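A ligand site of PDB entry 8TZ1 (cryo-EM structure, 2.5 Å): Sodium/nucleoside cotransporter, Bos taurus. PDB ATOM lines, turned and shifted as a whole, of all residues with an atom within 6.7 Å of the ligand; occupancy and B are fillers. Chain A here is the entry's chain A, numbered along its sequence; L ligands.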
ATOM      1  N   VAL A 313      -6.960 -18.643  30.712  1.00  0.00           N
ATOM      2  CA  VAL A 313      -7.086 -19.628  29.643  1.00  0.00           C
ATOM      3  C   VAL A 313      -5.745 -20.295  29.384  1.00  0.00           C
ATOM      4  O   VAL A 313      -5.669 -21.517  29.176  1.00  0.00           O
ATOM      5  CB  VAL A 313      -7.639 -18.964  28.375  1.00  0.00           C
ATOM      6  CG1 VAL A 313      -7.804 -19.985  27.265  1.00  0.00           C
ATOM      7  CG2 VAL A 313      -8.959 -18.283  28.669  1.00  0.00           C
ATOM      8  N   SER A 317      -5.067 -24.345  30.001  1.00  0.00           N
ATOM      9  CA  SER A 317      -4.607 -25.171  28.894  1.00  0.00           C
ATOM     10  C   SER A 317      -3.325 -25.897  29.263  1.00  0.00           C
ATOM     11  O   SER A 317      -3.145 -27.076  28.922  1.00  0.00           O
ATOM     12  CB  SER A 317      -4.403 -24.316  27.644  1.00  0.00           C
ATOM     13  OG  SER A 317      -5.562 -23.567  27.347  1.00  0.00           O
ATOM     14  N   ILE A 360     -12.792 -31.380  27.034  1.00  0.00           N
ATOM     15  CA  ILE A 360     -11.988 -30.990  25.885  1.00  0.00           C
ATOM     16  C   ILE A 360     -12.878 -30.301  24.859  1.00  0.00           C
ATOM     17  O   ILE A 360     -14.100 -30.499  24.824  1.00  0.00           O
ATOM     18  CB  ILE A 360     -11.262 -32.197  25.253  1.00  0.00           C
ATOM     19  CG1 ILE A 360     -10.525 -32.989  26.335  1.00  0.00           C
ATOM     20  CG2 ILE A 360     -10.271 -31.730  24.204  1.00  0.00           C
ATOM     21  CD1 ILE A 360      -9.956 -34.290  25.855  1.00  0.00           C
ATOM     22  N   GLY A 361     -12.261 -29.470  24.030  1.00  0.00           N
ATOM     23  CA  GLY A 361     -12.975 -28.720  23.029  1.00  0.00           C
ATOM     24  C   GLY A 361     -13.440 -29.584  21.868  1.00  0.00           C
ATOM     25  O   GLY A 361     -13.070 -30.746  21.709  1.00  0.00           O
ATOM     26  N   GLN A 362     -14.286 -28.974  21.029  1.00  0.00           N
ATOM     27  CA  GLN A 362     -14.863 -29.685  19.904  1.00  0.00           C
ATOM     28  C   GLN A 362     -13.811 -30.117  18.889  1.00  0.00           C
ATOM     29  O   GLN A 362     -13.974 -31.137  18.216  1.00  0.00           O
ATOM     30  CB  GLN A 362     -15.916 -28.819  19.224  1.00  0.00           C
ATOM     31  CG  GLN A 362     -15.354 -27.559  18.585  1.00  0.00           C
ATOM     32  CD  GLN A 362     -16.412 -26.523  18.288  1.00  0.00           C
ATOM     33  OE1 GLN A 362     -17.577 -26.868  18.065  1.00  0.00           O
ATOM     34  NE2 GLN A 362     -16.024 -25.263  18.281  1.00  0.00           N
ATOM     35  N   THR A 363     -12.731 -29.344  18.769  1.00  0.00           N
ATOM     36  CA  THR A 363     -11.728 -29.596  17.740  1.00  0.00           C
ATOM     37  C   THR A 363     -10.604 -30.522  18.198  1.00  0.00           C
ATOM     38  O   THR A 363      -9.842 -30.999  17.346  1.00  0.00           O
ATOM     39  CB  THR A 363     -11.119 -28.265  17.272  1.00  0.00           C
ATOM     40  OG1 THR A 363     -11.126 -27.328  18.355  1.00  0.00           O
ATOM     41  CG2 THR A 363     -11.896 -27.707  16.096  1.00  0.00           C
ATOM     42  N   GLU A 364     -10.487 -30.798  19.495  1.00  0.00           N
ATOM     43  CA  GLU A 364      -9.424 -31.665  20.011  1.00  0.00           C
ATOM     44  C   GLU A 364      -9.946 -32.943  20.634  1.00  0.00           C
ATOM     45  O   GLU A 364      -9.141 -33.801  21.017  1.00  0.00           O
ATOM     46  CB  GLU A 364      -8.590 -30.894  21.043  1.00  0.00           C
ATOM     47  CG  GLU A 364      -8.030 -29.583  20.542  1.00  0.00           C
ATOM     48  CD  GLU A 364      -8.810 -28.373  21.040  1.00  0.00           C
ATOM     49  OE1 GLU A 364      -9.295 -28.411  22.186  1.00  0.00           O
ATOM     50  OE2 GLU A 364      -8.949 -27.396  20.269  1.00  0.00           O
ATOM     51  N   ALA A 393     -15.143 -26.350  26.793  1.00  0.00           N
ATOM     52  CA  ALA A 393     -13.838 -26.859  27.151  1.00  0.00           C
ATOM     53  C   ALA A 393     -13.455 -26.393  28.545  1.00  0.00           C
ATOM     54  O   ALA A 393     -14.003 -25.422  29.080  1.00  0.00           O
ATOM     55  CB  ALA A 393     -12.787 -26.392  26.144  1.00  0.00           C
ATOM     56  N   GLY A 394     -12.508 -27.109  29.143  1.00  0.00           N
ATOM     57  CA  GLY A 394     -12.013 -26.740  30.454  1.00  0.00           C
ATOM     58  C   GLY A 394     -11.095 -25.537  30.458  1.00  0.00           C
ATOM     59  O   GLY A 394     -10.826 -24.985  31.538  1.00  0.00           O
ATOM     60  N   SER A 395     -10.611 -25.118  29.294  1.00  0.00           N
ATOM     61  CA  SER A 395      -9.733 -23.957  29.217  1.00  0.00           C
ATOM     62  C   SER A 395     -10.515 -22.656  29.356  1.00  0.00           C
ATOM     63  O   SER A 395     -10.029 -21.698  29.976  1.00  0.00           O
ATOM     64  CB  SER A 395      -8.956 -23.971  27.910  1.00  0.00           C
ATOM     65  OG  SER A 395      -9.819 -24.133  26.798  1.00  0.00           O
ATOM     66  N   VAL A 396     -11.730 -22.601  28.796  1.00  0.00           N
ATOM     67  CA  VAL A 396     -12.545 -21.397  28.871  1.00  0.00           C
ATOM     68  C   VAL A 396     -13.441 -21.363  30.103  1.00  0.00           C
ATOM     69  O   VAL A 396     -14.179 -20.391  30.300  1.00  0.00           O
ATOM     70  CB  VAL A 396     -13.410 -21.243  27.602  1.00  0.00           C
ATOM     71  CG1 VAL A 396     -12.533 -21.064  26.386  1.00  0.00           C
ATOM     72  CG2 VAL A 396     -14.325 -22.451  27.422  1.00  0.00           C
ATOM     73  N   TYR A 400     -15.412 -17.801  32.148  1.00  0.00           N
ATOM     74  CA  TYR A 400     -16.822 -17.673  32.469  1.00  0.00           C
ATOM     75  C   TYR A 400     -17.029 -17.457  33.957  1.00  0.00           C
ATOM     76  O   TYR A 400     -17.885 -16.670  34.370  1.00  0.00           O
ATOM     77  CB  TYR A 400     -17.585 -18.902  31.994  1.00  0.00           C
ATOM     78  CG  TYR A 400     -17.456 -19.161  30.509  1.00  0.00           C
ATOM     79  CD1 TYR A 400     -17.292 -18.115  29.612  1.00  0.00           C
ATOM     80  CD2 TYR A 400     -17.509 -20.449  30.005  1.00  0.00           C
ATOM     81  CE1 TYR A 400     -17.173 -18.350  28.264  1.00  0.00           C
ATOM     82  CE2 TYR A 400     -17.395 -20.697  28.656  1.00  0.00           C
ATOM     83  CZ  TYR A 400     -17.226 -19.632  27.784  1.00  0.00           C
ATOM     84  OH  TYR A 400     -17.107 -19.866  26.436  1.00  0.00           O
ATOM     85  N   LEU A 467      -5.515 -19.772  20.468  1.00  0.00           N
ATOM     86  CA  LEU A 467      -6.808 -19.792  21.143  1.00  0.00           C
ATOM     87  C   LEU A 467      -7.200 -18.406  21.622  1.00  0.00           C
ATOM     88  O   LEU A 467      -8.304 -17.927  21.335  1.00  0.00           O
ATOM     89  CB  LEU A 467      -6.756 -20.774  22.311  1.00  0.00           C
ATOM     90  CG  LEU A 467      -8.058 -21.431  22.759  1.00  0.00           C
ATOM     91  CD1 LEU A 467      -7.796 -22.261  23.992  1.00  0.00           C
ATOM     92  CD2 LEU A 467      -9.144 -20.414  23.022  1.00  0.00           C
ATOM     93  N   ASN A 470      -7.581 -15.753  18.600  1.00  0.00           N
ATOM     94  CA  ASN A 470      -8.851 -15.856  17.891  1.00  0.00           C
ATOM     95  C   ASN A 470     -10.005 -15.346  18.754  1.00  0.00           C
ATOM     96  O   ASN A 470     -10.931 -14.694  18.246  1.00  0.00           O
ATOM     97  CB  ASN A 470      -9.097 -17.296  17.461  1.00  0.00           C
ATOM     98  CG  ASN A 470      -8.354 -17.658  16.189  1.00  0.00           C
ATOM     99  OD1 ASN A 470      -8.841 -17.427  15.085  1.00  0.00           O
ATOM    100  ND2 ASN A 470      -7.171 -18.242  16.336  1.00  0.00           N
ATOM    101  N   ILE A 471      -9.978 -15.637  20.052  1.00  0.00           N
ATOM    102  CA  ILE A 471     -11.025 -15.170  20.953  1.00  0.00           C
ATOM    103  C   ILE A 471     -11.099 -13.644  20.926  1.00  0.00           C
ATOM    104  O   ILE A 471     -12.163 -13.045  20.770  1.00  0.00           O
ATOM    105  CB  ILE A 471     -10.791 -15.691  22.380  1.00  0.00           C
ATOM    106  CG1 ILE A 471     -11.236 -17.148  22.490  1.00  0.00           C
ATOM    107  CG2 ILE A 471     -11.509 -14.816  23.399  1.00  0.00           C
ATOM    108  CD1 ILE A 471     -10.907 -17.797  23.820  1.00  0.00           C
ATOM    109  N   ASN A 539     -20.723 -15.658  19.579  1.00  0.00           N
ATOM    110  CA  ASN A 539     -20.228 -16.816  20.376  1.00  0.00           C
ATOM    111  C   ASN A 539     -20.863 -16.726  21.776  1.00  0.00           C
ATOM    112  O   ASN A 539     -21.647 -15.778  21.976  1.00  0.00           O
ATOM    113  CB  ASN A 539     -18.705 -16.895  20.370  1.00  0.00           C
ATOM    114  CG  ASN A 539     -17.989 -15.652  20.850  1.00  0.00           C
ATOM    115  OD1 ASN A 539     -18.562 -14.832  21.566  1.00  0.00           O
ATOM    116  ND2 ASN A 539     -16.730 -15.483  20.472  1.00  0.00           N
ATOM    117  N   GLU A 540     -20.558 -17.653  22.687  1.00  0.00           N
ATOM    118  CA  GLU A 540     -21.105 -17.677  24.033  1.00  0.00           C
ATOM    119  C   GLU A 540     -20.326 -16.812  25.008  1.00  0.00           C
ATOM    120  O   GLU A 540     -20.742 -16.672  26.165  1.00  0.00           O
ATOM    121  CB  GLU A 540     -21.182 -19.120  24.559  1.00  0.00           C
ATOM    122  CG  GLU A 540     -19.844 -19.793  24.864  1.00  0.00           C
ATOM    123  CD  GLU A 540     -19.082 -20.199  23.616  1.00  0.00           C
ATOM    124  OE1 GLU A 540     -19.648 -20.099  22.506  1.00  0.00           O
ATOM    125  OE2 GLU A 540     -17.910 -20.615  23.738  1.00  0.00           O
ATOM    126  N   PHE A 541     -19.202 -16.227  24.593  1.00  0.00           N
ATOM    127  CA  PHE A 541     -18.526 -15.238  25.426  1.00  0.00           C
ATOM    128  C   PHE A 541     -19.382 -13.988  25.579  1.00  0.00           C
ATOM    129  O   PHE A 541     -19.444 -13.391  26.653  1.00  0.00           O
ATOM    130  CB  PHE A 541     -17.168 -14.871  24.830  1.00  0.00           C
ATOM    131  CG  PHE A 541     -16.010 -15.534  25.513  1.00  0.00           C
ATOM    132  CD1 PHE A 541     -15.620 -16.807  25.150  1.00  0.00           C
ATOM    133  CD2 PHE A 541     -15.306 -14.875  26.494  1.00  0.00           C
ATOM    134  CE1 PHE A 541     -14.537 -17.412  25.770  1.00  0.00           C
ATOM    135  CE2 PHE A 541     -14.233 -15.469  27.115  1.00  0.00           C
ATOM    136  CZ  PHE A 541     -13.852 -16.740  26.748  1.00  0.00           C
ATOM    137  N   GLY A 583     -22.413 -24.229  25.614  1.00  0.00           N
ATOM    138  CA  GLY A 583     -22.147 -24.941  24.388  1.00  0.00           C
ATOM    139  C   GLY A 583     -21.330 -24.105  23.425  1.00  0.00           C
ATOM    140  O   GLY A 583     -21.299 -22.873  23.518  1.00  0.00           O
ATOM    141  N   PHE A 584     -20.675 -24.803  22.497  1.00  0.00           N
ATOM    142  CA  PHE A 584     -19.909 -24.190  21.424  1.00  0.00           C
ATOM    143  C   PHE A 584     -20.699 -24.124  20.117  1.00  0.00           C
ATOM    144  O   PHE A 584     -20.096 -24.039  19.045  1.00  0.00           O
ATOM    145  CB  PHE A 584     -18.610 -24.950  21.201  1.00  0.00           C
ATOM    146  CG  PHE A 584     -17.526 -24.674  22.210  1.00  0.00           C
ATOM    147  CD1 PHE A 584     -17.725 -23.770  23.249  1.00  0.00           C
ATOM    148  CD2 PHE A 584     -16.300 -25.300  22.111  1.00  0.00           C
ATOM    149  CE1 PHE A 584     -16.720 -23.529  24.164  1.00  0.00           C
ATOM    150  CE2 PHE A 584     -15.297 -25.050  23.015  1.00  0.00           C
ATOM    151  CZ  PHE A 584     -15.508 -24.165  24.041  1.00  0.00           C
ATOM    152  N   ALA A 585     -22.024 -24.156  20.194  1.00  0.00           N
ATOM    153  CA  ALA A 585     -22.866 -24.208  19.008  1.00  0.00           C
ATOM    154  C   ALA A 585     -23.150 -22.795  18.524  1.00  0.00           C
ATOM    155  O   ALA A 585     -23.916 -22.050  19.152  1.00  0.00           O
ATOM    156  CB  ALA A 585     -24.165 -24.954  19.314  1.00  0.00           C
ATOM    157  N   ASN A 586     -22.528 -22.423  17.407  1.00  0.00           N
ATOM    158  CA  ASN A 586     -22.820 -21.159  16.741  1.00  0.00           C
ATOM    159  C   ASN A 586     -22.569 -21.345  15.258  1.00  0.00           C
ATOM    160  O   ASN A 586     -21.794 -22.217  14.850  1.00  0.00           O
ATOM    161  CB  ASN A 586     -21.989 -20.008  17.302  1.00  0.00           C
ATOM    162  CG  ASN A 586     -20.503 -20.319  17.365  1.00  0.00           C
ATOM    163  OD1 ASN A 586     -19.809 -20.295  16.349  1.00  0.00           O
ATOM    164  ND2 ASN A 586     -20.018 -20.615  18.557  1.00  0.00           N
ATOM    165  N   SER A 589     -18.907 -21.463  14.104  1.00  0.00           N
ATOM    166  CA  SER A 589     -18.105 -22.650  14.416  1.00  0.00           C
ATOM    167  C   SER A 589     -18.305 -23.771  13.411  1.00  0.00           C
ATOM    168  O   SER A 589     -17.533 -24.729  13.415  1.00  0.00           O
ATOM    169  CB  SER A 589     -18.445 -23.152  15.821  1.00  0.00           C
ATOM    170  OG  SER A 589     -17.969 -22.259  16.815  1.00  0.00           O
ATOM    171  N   ILE A 592     -15.087 -24.152  10.986  1.00  0.00           N
ATOM    172  CA  ILE A 592     -13.848 -24.619  11.587  1.00  0.00           C
ATOM    173  C   ILE A 592     -13.986 -26.074  12.024  1.00  0.00           C
ATOM    174  O   ILE A 592     -13.034 -26.860  11.946  1.00  0.00           O
ATOM    175  CB  ILE A 592     -13.420 -23.714  12.756  1.00  0.00           C
ATOM    176  CG1 ILE A 592     -14.404 -23.819  13.930  1.00  0.00           C
ATOM    177  CG2 ILE A 592     -13.331 -22.271  12.293  1.00  0.00           C
ATOM    178  CD1 ILE A 592     -13.942 -24.741  15.031  1.00  0.00           C
HETATM  179  N1  LIG L   1     -13.062 -21.944  21.468  1.00  0.00           N
HETATM  180  N2  LIG L   1     -12.531 -23.178  21.177  1.00  0.00           N
HETATM  181  C1  LIG L   1     -11.917 -23.603  22.235  1.00  0.00           C
HETATM  182  N3  LIG L   1     -10.418 -25.232  23.578  1.00  0.00           N
HETATM  183  O1  LIG L   1     -11.188 -25.747  21.487  1.00  0.00           O
HETATM  184  N4  LIG L   1     -12.042 -22.666  23.189  1.00  0.00           N
HETATM  185  C2  LIG L   1     -12.760 -21.649  22.690  1.00  0.00           C
HETATM  186  C3  LIG L   1     -11.162 -24.957  22.361  1.00  0.00           C
HETATM  187  C4  LIG L   1     -13.763 -21.201  20.628  1.00  0.00           C
HETATM  188  C5  LIG L   1     -15.223 -21.817  20.396  1.00  0.00           C
HETATM  189  O2  LIG L   1     -15.570 -21.812  18.891  1.00  0.00           O
HETATM  190  C6  LIG L   1     -15.982 -21.086  20.981  1.00  0.00           C
HETATM  191  O3  LIG L   1     -17.298 -21.001  20.218  1.00  0.00           O
HETATM  192  C7  LIG L   1     -15.230 -19.601  20.985  1.00  0.00           C
HETATM  193  O4  LIG L   1     -14.002 -19.848  21.217  1.00  0.00           O
HETATM  194  C8  LIG L   1     -15.804 -18.748  22.118  1.00  0.00           C
HETATM  195  O5  LIG L   1     -15.186 -19.140  23.335  1.00  0.00           O
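The side-chain carboxylate (OE2) of Glu 364 sits close to an oxygen (O1) of the ligand, at 3.0 Å. Gly 361 touches the ligand (CA to O1, 3.8 Å). NE2 of Gln 362 touches O2 of the ligand (3.5 Å). Thr 363 touches the ligand (OG1 to O1, 3.5 Å). CB of Ala 393 touches N3 of the ligand, at 3.7 Å. Val 396 touches the ligand (CG1 to N4, 3.6 Å). Tyr 400 touches the ligand. Leu 467 touches the ligand. Asn 539 touches the ligand. Phe 541 touches the ligand. CE2 of Phe 584 touches C1 of the ligand, at 3.8 Å. Hydrophobic or aromatic side chains within 4 Å of the ligand: Ala 393, Val 396, Leu 467, Phe 541 and Phe 584. Of the 24 residues printed, 15 come within 4 Å of the ligand. The nearest printed residue that does not touch the ligand is Ile 471 (4.1 Å).
The side-chain amide oxygen (OD1) of Asn 539 sits close to the backbone NH (N) of Phe 541, 3.4 Å away. The side-chain carboxylate (OE2) of Glu 364 lies within hydrogen-bond range of the side-chain hydroxyl (OG1) of Thr 363. The side-chain carboxylate (OE2) of Glu 540 is in hydrogen-bond range of the side-chain hydroxyl (OH) of Tyr 400. The side-chain amide oxygen (OD1) of Asn 586 lies within hydrogen-bond range of the backbone NH (N) of Ser 589 (2.7 Å). ND2 of Asn 586 is in hydrogen-bond range of O of Phe 584 (3.5 Å).
O5 of the ligand lies within hydrogen-bond range of OE2 of Glu 540 (3.1 Å). OG of Ser 589 sits at hydrogen-bond distance from O2 of the ligand, at 3.2 Å. The side-chain amide nitrogen (ND2) of Asn 586 lies within hydrogen-bond range of an oxygen (O3) of the ligand (3.2 Å). A nitrogen (N3) of the ligand is in hydrogen-bond range of the side-chain hydroxyl of Ser 395 (3.5 Å).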
